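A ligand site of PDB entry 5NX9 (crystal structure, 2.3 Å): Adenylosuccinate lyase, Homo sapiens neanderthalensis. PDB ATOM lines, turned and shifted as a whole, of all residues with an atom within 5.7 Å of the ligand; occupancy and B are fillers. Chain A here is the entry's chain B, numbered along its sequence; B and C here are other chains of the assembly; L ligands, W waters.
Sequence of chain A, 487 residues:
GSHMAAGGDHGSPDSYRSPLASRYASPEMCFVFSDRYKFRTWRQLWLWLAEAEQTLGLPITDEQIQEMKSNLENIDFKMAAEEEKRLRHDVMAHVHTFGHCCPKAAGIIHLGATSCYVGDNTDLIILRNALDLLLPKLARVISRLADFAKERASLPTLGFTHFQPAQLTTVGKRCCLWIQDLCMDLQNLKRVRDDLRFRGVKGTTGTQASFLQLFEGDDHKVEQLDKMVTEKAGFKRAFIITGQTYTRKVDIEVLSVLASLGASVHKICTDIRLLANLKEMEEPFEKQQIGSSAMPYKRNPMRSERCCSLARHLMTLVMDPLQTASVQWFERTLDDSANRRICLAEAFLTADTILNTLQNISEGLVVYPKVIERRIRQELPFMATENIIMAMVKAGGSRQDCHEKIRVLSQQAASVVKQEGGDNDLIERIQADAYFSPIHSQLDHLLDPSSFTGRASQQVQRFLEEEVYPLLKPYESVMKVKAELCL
An oxygen (O3) of the ligand is in hydrogen-bond range of the side-chain hydroxyl (OG) of Ser 337 (2.5 Å). OH of Tyr 24 of chain B sits at hydrogen-bond distance from O2 of the ligand, 2.5 Å away. An oxygen (O9) of the ligand lies within hydrogen-bond range of the backbone NH of Ser 115 (3.0 Å). An oxygen (O9) of the ligand lies within hydrogen-bond range of the side-chain hydroxyl (OG) of Ser 115 (2.6 Å). The side-chain hydroxyl (OG1) of Thr 161 of chain C sits at hydrogen-bond distance from an oxygen (O7) of the ligand (2.6 Å). O10 of the ligand sits at hydrogen-bond distance from O of Arg 88 (2.6 Å). O8 of the ligand is in hydrogen-bond range of NE2 of His 89 (2.7 Å). NE2 of Gln 244 sits at hydrogen-bond distance from O7 of the ligand (2.8 Å). NE of Arg 341 is in salt-bridge range of O3 of the ligand, 2.8 Å away. The guanidinium group of Arg 23 of chain B lies within salt-bridge range of an oxygen (O2) of the ligand (2.9 Å). An oxygen (O9) of the ligand is in hydrogen-bond range of the side-chain hydroxyl (OG1) of Thr 114, at 3.0 Å. An oxygen (O2) of the ligand lies within salt-bridge range of the guanidinium group (NE) of Arg 306 of chain B (3.1 Å). An oxygen (O11) of the ligand lies within hydrogen-bond range of the backbone NH of Asp 90 (3.2 Å). N5 of the ligand sits at hydrogen-bond distance from NE2 of His 162 of chain C, at 3.3 Å. The backbone NH of Ala 338 lies within hydrogen-bond range of an oxygen (O3) of the ligand, 3.4 Å away. ND2 of Asn 300 of chain B sits at hydrogen-bond distance from O6 of the ligand (3.4 Å).
OH of Tyr 24 of chain B sits close to NE of Arg 341 (3.3 Å). OH of Tyr 24 of chain B lies within hydrogen-bond range of NE of Arg 23 of chain B (3.4 Å). The side-chain amide oxygen (OE1) of Gln 244 is in hydrogen-bond range of the guanidinium group (NH1) of Arg 332 (2.9 Å). The backbone carbonyl oxygen (O) of Thr 204 lies within hydrogen-bond range of the side-chain amide nitrogen (NE2) of Gln 244 (2.8 Å). The guanidinium group (NH2) of Arg 341 lies within salt-bridge range of the side-chain carboxylate (OD2) of Asp 90 (3.0 Å). NH1 of Arg 23 of chain B lies within salt-bridge range of OE1 of Glu 84 (2.8 Å). The backbone carbonyl oxygen (O) of Arg 332 lies within hydrogen-bond range of the backbone NH (N) of His 162 of chain C (3.0 Å). NH1 of Arg 332 lies within hydrogen-bond range of SG of Cys 116 (3.2 Å).
Merely in contact with the ligand: Met 302 of chain B (3.0 Å), Leu 334 (3.4 Å) and Arg 332 (3.7 Å). Hydrophobic or aromatic side chains that line the ligand: His 89, Leu 334, Tyr 24 of chain B, Met 302 of chain B and His 162 of chain C. Of the 26 residues printed, 18 come within 4 Å of the ligand. The nearest printed residue that does not touch the ligand is Thr 204 (4.1 Å).
Water W2 lies within hydrogen-bond range of the side-chain hydroxyl of Thr 114 (2.8 Å), the backbone NH of Cys 116 (2.9 Å), a nitrogen (N3) of the ligand (3.0 Å), the side-chain amide oxygen of Gln 244 (3.1 Å) and the backbone NH of Ser 115 (3.3 Å). Water W4 lies within hydrogen-bond range of OG1 of Thr 161 of chain C (3.0 Å) and O6 of the ligand (3.4 Å).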
ATOM      1  N   GLU A  84      -9.035  -2.480  13.799  1.00  0.00           N
ATOM      2  CA  GLU A  84      -8.560  -1.505  14.774  1.00  0.00           C
ATOM      3  C   GLU A  84      -7.608  -2.165  15.790  1.00  0.00           C
ATOM      4  O   GLU A  84      -6.599  -1.563  16.179  1.00  0.00           O
ATOM      5  CB  GLU A  84      -9.717  -0.778  15.489  1.00  0.00           C
ATOM      6  CG  GLU A  84      -9.199   0.304  16.416  1.00  0.00           C
ATOM      7  CD  GLU A  84     -10.267   1.305  16.882  1.00  0.00           C
ATOM      8  OE1 GLU A  84      -9.899   2.188  17.693  1.00  0.00           O
ATOM      9  OE2 GLU A  84     -11.448   1.222  16.446  1.00  0.00           O
ATOM     10  N   ARG A  88      -4.321  -0.332  15.365  1.00  0.00           N
ATOM     11  CA  ARG A  88      -4.379   0.677  16.446  1.00  0.00           C
ATOM     12  C   ARG A  88      -4.737   2.064  15.919  1.00  0.00           C
ATOM     13  O   ARG A  88      -4.268   3.078  16.440  1.00  0.00           O
ATOM     14  CB  ARG A  88      -3.054   0.747  17.239  1.00  0.00           C
ATOM     15  CG  ARG A  88      -2.455  -0.565  17.667  1.00  0.00           C
ATOM     16  CD  ARG A  88      -3.300  -1.315  18.640  1.00  0.00           C
ATOM     17  NE  ARG A  88      -2.369  -2.090  19.452  1.00  0.00           N
ATOM     18  CZ  ARG A  88      -2.703  -2.877  20.460  1.00  0.00           C
ATOM     19  NH1 ARG A  88      -3.988  -3.071  20.810  1.00  0.00           N
ATOM     20  NH2 ARG A  88      -1.730  -3.531  21.120  1.00  0.00           N
ATOM     21  N   HIS A  89      -5.572   2.103  14.879  1.00  0.00           N
ATOM     22  CA  HIS A  89      -5.959   3.355  14.240  1.00  0.00           C
ATOM     23  C   HIS A  89      -7.387   3.229  13.763  1.00  0.00           C
ATOM     24  O   HIS A  89      -7.646   2.494  12.816  1.00  0.00           O
ATOM     25  CB  HIS A  89      -5.021   3.640  13.063  1.00  0.00           C
ATOM     26  CG  HIS A  89      -4.991   5.067  12.651  1.00  0.00           C
ATOM     27  ND1 HIS A  89      -6.025   5.665  11.954  1.00  0.00           N
ATOM     28  CD2 HIS A  89      -4.068   6.028  12.855  1.00  0.00           C
ATOM     29  CE1 HIS A  89      -5.717   6.930  11.738  1.00  0.00           C
ATOM     30  NE2 HIS A  89      -4.542   7.184  12.280  1.00  0.00           N
ATOM     31  N   ASP A  90      -8.325   3.917  14.430  1.00  0.00           N
ATOM     32  CA  ASP A  90      -9.748   3.763  14.103  1.00  0.00           C
ATOM     33  C   ASP A  90     -10.108   4.130  12.656  1.00  0.00           C
ATOM     34  O   ASP A  90     -10.833   3.396  11.981  1.00  0.00           O
ATOM     35  CB  ASP A  90     -10.689   4.471  15.128  1.00  0.00           C
ATOM     36  CG  ASP A  90     -10.410   5.984  15.309  1.00  0.00           C
ATOM     37  OD1 ASP A  90      -9.413   6.541  14.782  1.00  0.00           O
ATOM     38  OD2 ASP A  90     -11.231   6.636  16.029  1.00  0.00           O
ATOM     39  N   VAL A  91      -9.572   5.236  12.161  1.00  0.00           N
ATOM     40  CA  VAL A  91      -9.906   5.697  10.808  1.00  0.00           C
ATOM     41  C   VAL A  91      -9.393   4.754   9.740  1.00  0.00           C
ATOM     42  O   VAL A  91     -10.113   4.443   8.786  1.00  0.00           O
ATOM     43  CB  VAL A  91      -9.456   7.160  10.568  1.00  0.00           C
ATOM     44  CG1 VAL A  91      -9.671   7.572   9.124  1.00  0.00           C
ATOM     45  CG2 VAL A  91     -10.238   8.080  11.490  1.00  0.00           C
ATOM     46  N   MET A  92      -8.164   4.267   9.892  1.00  0.00           N
ATOM     47  CA  MET A  92      -7.578   3.376   8.873  1.00  0.00           C
ATOM     48  C   MET A  92      -8.279   2.031   8.903  1.00  0.00           C
ATOM     49  O   MET A  92      -8.467   1.428   7.846  1.00  0.00           O
ATOM     50  CB  MET A  92      -6.072   3.194   9.055  1.00  0.00           C
ATOM     51  CG  MET A  92      -5.267   4.392   8.551  1.00  0.00           C
ATOM     52  SD  MET A  92      -5.593   4.933   6.815  1.00  0.00           S
ATOM     53  CE  MET A  92      -5.753   6.666   7.207  1.00  0.00           C
ATOM     54  N   HIS A 110     -10.404   8.216   0.938  1.00  0.00           N
ATOM     55  CA  HIS A 110      -9.549   9.028   1.816  1.00  0.00           C
ATOM     56  C   HIS A 110      -8.415   9.741   1.077  1.00  0.00           C
ATOM     57  O   HIS A 110      -7.446  10.209   1.697  1.00  0.00           O
ATOM     58  CB  HIS A 110      -8.959   8.160   2.943  1.00  0.00           C
ATOM     59  CG  HIS A 110      -8.603   8.917   4.187  1.00  0.00           C
ATOM     60  ND1 HIS A 110      -9.530   9.604   4.931  1.00  0.00           N
ATOM     61  CD2 HIS A 110      -7.413   9.074   4.810  1.00  0.00           C
ATOM     62  CE1 HIS A 110      -8.922  10.176   5.960  1.00  0.00           C
ATOM     63  NE2 HIS A 110      -7.639   9.868   5.908  1.00  0.00           N
ATOM     64  N   ALA A 113      -6.699  13.133   2.194  1.00  0.00           N
ATOM     65  CA  ALA A 113      -7.227  13.588   3.490  1.00  0.00           C
ATOM     66  C   ALA A 113      -6.436  13.055   4.672  1.00  0.00           C
ATOM     67  O   ALA A 113      -5.771  12.037   4.575  1.00  0.00           O
ATOM     68  CB  ALA A 113      -8.689  13.167   3.605  1.00  0.00           C
ATOM     69  N   THR A 114      -6.545  13.747   5.796  1.00  0.00           N
ATOM     70  CA  THR A 114      -6.100  13.223   7.083  1.00  0.00           C
ATOM     71  C   THR A 114      -7.317  12.722   7.843  1.00  0.00           C
ATOM     72  O   THR A 114      -8.461  12.980   7.462  1.00  0.00           O
ATOM     73  CB  THR A 114      -5.309  14.315   7.872  1.00  0.00           C
ATOM     74  OG1 THR A 114      -4.682  13.729   9.012  1.00  0.00           O
ATOM     75  CG2 THR A 114      -6.227  15.459   8.336  1.00  0.00           C
ATOM     76  N   SER A 115      -7.081  11.981   8.910  1.00  0.00           N
ATOM     77  CA  SER A 115      -8.149  11.301   9.651  1.00  0.00           C
ATOM     78  C   SER A 115      -9.250  12.253  10.112  1.00  0.00           C
ATOM     79  O   SER A 115     -10.424  11.863  10.083  1.00  0.00           O
ATOM     80  CB  SER A 115      -7.565  10.600  10.874  1.00  0.00           C
ATOM     81  OG  SER A 115      -6.651   9.613  10.480  1.00  0.00           O
ATOM     82  N   CYS A 116      -8.884  13.475  10.516  1.00  0.00           N
ATOM     83  CA  CYS A 116      -9.878  14.455  10.952  1.00  0.00           C
ATOM     84  C   CYS A 116     -10.856  14.890   9.870  1.00  0.00           C
ATOM     85  O   CYS A 116     -11.906  15.453  10.204  1.00  0.00           O
ATOM     86  CB  CYS A 116      -9.212  15.698  11.537  1.00  0.00           C
ATOM     87  SG  CYS A 116      -8.577  15.448  13.203  1.00  0.00           S
ATOM     88  N   THR A 204      -3.113  17.429   6.745  1.00  0.00           N
ATOM     89  CA  THR A 204      -2.569  16.984   8.030  1.00  0.00           C
ATOM     90  C   THR A 204      -2.312  18.122   9.038  1.00  0.00           C
ATOM     91  O   THR A 204      -2.504  17.920  10.239  1.00  0.00           O
ATOM     92  CB  THR A 204      -1.236  16.227   7.808  1.00  0.00           C
ATOM     93  OG1 THR A 204      -1.505  15.102   6.977  1.00  0.00           O
ATOM     94  CG2 THR A 204      -0.625  15.745   9.110  1.00  0.00           C
ATOM     95  N   GLN A 244      -4.675  20.794  12.251  1.00  0.00           N
ATOM     96  CA  GLN A 244      -5.266  19.527  11.851  1.00  0.00           C
ATOM     97  C   GLN A 244      -6.779  19.488  12.161  1.00  0.00           C
ATOM     98  O   GLN A 244      -7.552  18.933  11.382  1.00  0.00           O
ATOM     99  CB  GLN A 244      -4.563  18.391  12.550  1.00  0.00           C
ATOM    100  CG  GLN A 244      -4.968  17.032  12.035  1.00  0.00           C
ATOM    101  CD  GLN A 244      -4.070  15.945  12.588  1.00  0.00           C
ATOM    102  OE1 GLN A 244      -4.379  15.332  13.617  1.00  0.00           O
ATOM    103  NE2 GLN A 244      -2.950  15.711  11.930  1.00  0.00           N
ATOM    104  N   ARG A 332      -2.140  20.483  16.755  1.00  0.00           N
ATOM    105  CA  ARG A 332      -3.014  19.468  17.367  1.00  0.00           C
ATOM    106  C   ARG A 332      -2.219  18.520  18.235  1.00  0.00           C
ATOM    107  O   ARG A 332      -1.173  18.043  17.816  1.00  0.00           O
ATOM    108  CB  ARG A 332      -3.671  18.622  16.266  1.00  0.00           C
ATOM    109  CG  ARG A 332      -4.807  17.794  16.738  1.00  0.00           C
ATOM    110  CD  ARG A 332      -4.445  16.380  17.029  1.00  0.00           C
ATOM    111  NE  ARG A 332      -5.651  15.808  17.603  1.00  0.00           N
ATOM    112  CZ  ARG A 332      -6.640  15.272  16.901  1.00  0.00           C
ATOM    113  NH1 ARG A 332      -6.534  15.122  15.582  1.00  0.00           N
ATOM    114  NH2 ARG A 332      -7.714  14.825  17.520  1.00  0.00           N
ATOM    115  N   LEU A 334      -3.222  14.756  20.442  1.00  0.00           N
ATOM    116  CA  LEU A 334      -4.292  13.767  20.561  1.00  0.00           C
ATOM    117  C   LEU A 334      -4.877  13.552  21.968  1.00  0.00           C
ATOM    118  O   LEU A 334      -5.755  12.696  22.155  1.00  0.00           O
ATOM    119  CB  LEU A 334      -3.915  12.398  19.958  1.00  0.00           C
ATOM    120  CG  LEU A 334      -4.881  12.169  18.754  1.00  0.00           C
ATOM    121  CD1 LEU A 334      -4.132  12.691  17.540  1.00  0.00           C
ATOM    122  CD2 LEU A 334      -5.430  10.761  18.506  1.00  0.00           C
ATOM    123  N   SER A 337      -8.787  13.573  22.336  1.00  0.00           N
ATOM    124  CA  SER A 337      -9.664  12.645  21.640  1.00  0.00           C
ATOM    125  C   SER A 337     -10.570  11.835  22.568  1.00  0.00           C
ATOM    126  O   SER A 337     -11.773  11.828  22.391  1.00  0.00           O
ATOM    127  CB  SER A 337      -8.861  11.722  20.731  1.00  0.00           C
ATOM    128  OG  SER A 337      -9.741  10.816  20.123  1.00  0.00           O
ATOM    129  N   ALA A 338      -9.996  11.136  23.522  1.00  0.00           N
ATOM    130  CA  ALA A 338     -10.797  10.236  24.373  1.00  0.00           C
ATOM    131  C   ALA A 338     -11.744  11.045  25.241  1.00  0.00           C
ATOM    132  O   ALA A 338     -12.899  10.659  25.436  1.00  0.00           O
ATOM    133  CB  ALA A 338      -9.886   9.384  25.245  1.00  0.00           C
ATOM    134  N   ARG A 341     -14.804  12.048  23.197  1.00  0.00           N
ATOM    135  CA  ARG A 341     -15.711  10.922  23.035  1.00  0.00           C
ATOM    136  C   ARG A 341     -16.721  10.837  24.195  1.00  0.00           C
ATOM    137  O   ARG A 341     -17.854  10.382  24.011  1.00  0.00           O
ATOM    138  CB  ARG A 341     -14.958   9.602  22.992  1.00  0.00           C
ATOM    139  CG  ARG A 341     -14.125   9.329  21.764  1.00  0.00           C
ATOM    140  CD  ARG A 341     -13.391   8.000  21.928  1.00  0.00           C
ATOM    141  NE  ARG A 341     -12.296   7.859  20.987  1.00  0.00           N
ATOM    142  CZ  ARG A 341     -12.410   7.427  19.729  1.00  0.00           C
ATOM    143  NH1 ARG A 341     -13.591   7.091  19.229  1.00  0.00           N
ATOM    144  NH2 ARG A 341     -11.325   7.359  18.953  1.00  0.00           N
ATOM    145  N   ARG B  23     -14.410   0.776  24.699  1.00  0.00           N
ATOM    146  CA  ARG B  23     -13.019   1.011  24.243  1.00  0.00           C
ATOM    147  C   ARG B  23     -11.970   0.766  25.310  1.00  0.00           C
ATOM    148  O   ARG B  23     -10.911   0.276  24.992  1.00  0.00           O
ATOM    149  CB  ARG B  23     -12.849   2.449  23.718  1.00  0.00           C
ATOM    150  CG  ARG B  23     -13.253   2.643  22.291  1.00  0.00           C
ATOM    151  CD  ARG B  23     -13.119   4.119  21.877  1.00  0.00           C
ATOM    152  NE  ARG B  23     -11.738   4.480  21.555  1.00  0.00           N
ATOM    153  CZ  ARG B  23     -11.102   4.107  20.427  1.00  0.00           C
ATOM    154  NH1 ARG B  23     -11.683   3.361  19.497  1.00  0.00           N
ATOM    155  NH2 ARG B  23      -9.844   4.481  20.243  1.00  0.00           N
ATOM    156  N   TYR B  24     -12.235   1.163  26.547  1.00  0.00           N
ATOM    157  CA  TYR B  24     -11.149   1.530  27.470  1.00  0.00           C
ATOM    158  C   TYR B  24     -10.947   0.618  28.696  1.00  0.00           C
ATOM    159  O   TYR B  24      -9.866   0.108  28.902  1.00  0.00           O
ATOM    160  CB  TYR B  24     -11.343   2.959  27.932  1.00  0.00           C
ATOM    161  CG  TYR B  24     -11.230   3.990  26.829  1.00  0.00           C
ATOM    162  CD1 TYR B  24     -10.180   3.944  25.903  1.00  0.00           C
ATOM    163  CD2 TYR B  24     -12.152   5.036  26.740  1.00  0.00           C
ATOM    164  CE1 TYR B  24     -10.082   4.881  24.899  1.00  0.00           C
ATOM    165  CE2 TYR B  24     -12.048   5.993  25.729  1.00  0.00           C
ATOM    166  CZ  TYR B  24     -11.022   5.906  24.817  1.00  0.00           C
ATOM    167  OH  TYR B  24     -10.936   6.851  23.841  1.00  0.00           O
ATOM    168  N   ASN B 300       4.439   8.433  17.403  1.00  0.00           N
ATOM    169  CA  ASN B 300       3.548   9.270  18.210  1.00  0.00           C
ATOM    170  C   ASN B 300       3.336   8.679  19.590  1.00  0.00           C
ATOM    171  O   ASN B 300       3.086   7.496  19.714  1.00  0.00           O
ATOM    172  CB  ASN B 300       2.207   9.435  17.499  1.00  0.00           C
ATOM    173  CG  ASN B 300       2.302  10.196  16.186  1.00  0.00           C
ATOM    174  OD1 ASN B 300       3.132  11.100  16.032  1.00  0.00           O
ATOM    175  ND2 ASN B 300       1.432   9.873  15.260  1.00  0.00           N
ATOM    176  N   MET B 302       0.996   8.038  21.525  1.00  0.00           N
ATOM    177  CA  MET B 302      -0.453   7.983  21.491  1.00  0.00           C
ATOM    178  C   MET B 302      -1.046   7.495  22.841  1.00  0.00           C
ATOM    179  O   MET B 302      -2.077   8.004  23.282  1.00  0.00           O
ATOM    180  CB  MET B 302      -0.878   7.077  20.310  1.00  0.00           C
ATOM    181  CG  MET B 302      -2.371   6.851  20.188  1.00  0.00           C
ATOM    182  SD  MET B 302      -3.293   8.414  20.031  1.00  0.00           S
ATOM    183  CE  MET B 302      -4.447   8.345  21.403  1.00  0.00           C
ATOM    184  N   ARG B 306      -3.571   9.524  25.357  1.00  0.00           N
ATOM    185  CA  ARG B 306      -4.827   9.007  25.843  1.00  0.00           C
ATOM    186  C   ARG B 306      -4.918   9.131  27.365  1.00  0.00           C
ATOM    187  O   ARG B 306      -5.994   9.468  27.912  1.00  0.00           O
ATOM    188  CB  ARG B 306      -5.003   7.547  25.423  1.00  0.00           C
ATOM    189  CG  ARG B 306      -6.323   6.922  25.849  1.00  0.00           C
ATOM    190  CD  ARG B 306      -6.434   5.497  25.270  1.00  0.00           C
ATOM    191  NE  ARG B 306      -6.518   5.525  23.818  1.00  0.00           N
ATOM    192  CZ  ARG B 306      -5.761   4.828  22.950  1.00  0.00           C
ATOM    193  NH1 ARG B 306      -4.794   4.017  23.349  1.00  0.00           N
ATOM    194  NH2 ARG B 306      -5.977   4.984  21.656  1.00  0.00           N
ATOM    195  N   THR C 161       2.091  17.830  15.071  1.00  0.00           N
ATOM    196  CA  THR C 161       0.925  17.132  15.556  1.00  0.00           C
ATOM    197  C   THR C 161       1.432  16.022  16.458  1.00  0.00           C
ATOM    198  O   THR C 161       2.454  15.438  16.163  1.00  0.00           O
ATOM    199  CB  THR C 161       0.076  16.545  14.389  1.00  0.00           C
ATOM    200  OG1 THR C 161       0.868  15.624  13.629  1.00  0.00           O
ATOM    201  CG2 THR C 161      -0.397  17.637  13.484  1.00  0.00           C
ATOM    202  N   HIS C 162       0.732  15.769  17.563  1.00  0.00           N
ATOM    203  CA  HIS C 162       1.278  14.990  18.685  1.00  0.00           C
ATOM    204  C   HIS C 162       2.640  15.533  19.171  1.00  0.00           C
ATOM    205  O   HIS C 162       3.421  14.805  19.773  1.00  0.00           O
ATOM    206  CB  HIS C 162       1.488  13.513  18.316  1.00  0.00           C
ATOM    207  CG  HIS C 162       0.326  12.860  17.637  1.00  0.00           C
ATOM    208  ND1 HIS C 162      -0.336  11.783  18.199  1.00  0.00           N
ATOM    209  CD2 HIS C 162      -0.207  13.034  16.403  1.00  0.00           C
ATOM    210  CE1 HIS C 162      -1.248  11.342  17.348  1.00  0.00           C
ATOM    211  NE2 HIS C 162      -1.202  12.087  16.264  1.00  0.00           N
ATOM    212  N   ALA C 166       5.658  17.240  11.460  1.00  0.00           N
ATOM    213  CA  ALA C 166       4.533  17.059  10.529  1.00  0.00           C
ATOM    214  C   ALA C 166       4.644  18.041   9.358  1.00  0.00           C
ATOM    215  O   ALA C 166       5.484  18.943   9.387  1.00  0.00           O
ATOM    216  CB  ALA C 166       3.215  17.262  11.272  1.00  0.00           C
HETATM  217  P1  LIG L   1      -8.501   7.605  21.515  1.00  0.00           P
HETATM  218  O1  LIG L   1      -7.312   8.214  22.212  1.00  0.00           O
HETATM  219  O2  LIG L   1      -9.056   6.419  22.286  1.00  0.00           O
HETATM  220  O3  LIG L   1      -9.583   8.636  21.283  1.00  0.00           O
HETATM  221  O4  LIG L   1      -8.007   7.038  20.057  1.00  0.00           O
HETATM  222  C1  LIG L   1      -7.274   7.921  19.219  1.00  0.00           C
HETATM  223  C2  LIG L   1      -7.350   7.316  17.837  1.00  0.00           C
HETATM  224  O5  LIG L   1      -7.063   8.204  16.938  1.00  0.00           O
HETATM  225  C3  LIG L   1      -5.929   7.623  16.134  1.00  0.00           C
HETATM  226  N1  LIG L   1      -5.103   8.621  15.665  1.00  0.00           N
HETATM  227  C4  LIG L   1      -5.522   9.748  14.997  1.00  0.00           C
HETATM  228  N2  LIG L   1      -6.735  10.260  14.654  1.00  0.00           N
HETATM  229  C5  LIG L   1      -6.787  11.434  14.012  1.00  0.00           C
HETATM  230  N3  LIG L   1      -5.681  12.132  13.663  1.00  0.00           N
HETATM  231  C6  LIG L   1      -4.465  11.669  13.965  1.00  0.00           C
HETATM  232  N4  LIG L   1      -3.276  12.418  13.602  1.00  0.00           N
HETATM  233  C7  LIG L   1      -2.197  11.865  12.752  1.00  0.00           C
HETATM  234  C8  LIG L   1      -0.922  12.705  12.895  1.00  0.00           C
HETATM  235  C9  LIG L   1      -2.627  11.835  11.259  1.00  0.00           C
HETATM  236  C10 LIG L   1      -3.657  10.722  10.903  1.00  0.00           C
HETATM  237  O6  LIG L   1       0.205  12.163  13.084  1.00  0.00           O
HETATM  238  O7  LIG L   1      -0.957  13.969  12.841  1.00  0.00           O
HETATM  239  O8  LIG L   1      -3.668   9.621  11.535  1.00  0.00           O
HETATM  240  O9  LIG L   1      -4.480  10.878   9.936  1.00  0.00           O
HETATM  241  C11 LIG L   1      -4.357  10.453  14.670  1.00  0.00           C
HETATM  242  N5  LIG L   1      -3.304   9.742  15.122  1.00  0.00           N
HETATM  243  C12 LIG L   1      -3.771   8.642  15.715  1.00  0.00           C
HETATM  244  C13 LIG L   1      -5.262   6.650  17.155  1.00  0.00           C
HETATM  245  O10 LIG L   1      -4.412   5.685  16.426  1.00  0.00           O
HETATM  246  C14 LIG L   1      -6.249   6.100  17.754  1.00  0.00           C
HETATM  247  O11 LIG L   1      -6.895   4.992  17.033  1.00  0.00           O
HETATM  248  O   HOH W   1      -2.370   7.481   9.169  1.00  0.00           O
HETATM  249  O   HOH W   2      -6.190  14.043  11.395  1.00  0.00           O
HETATM  250  O   HOH W   3      -0.647   7.302  16.284  1.00  0.00           O
HETATM  251  O   HOH W   4       3.152  13.706  13.553  1.00  0.00           O
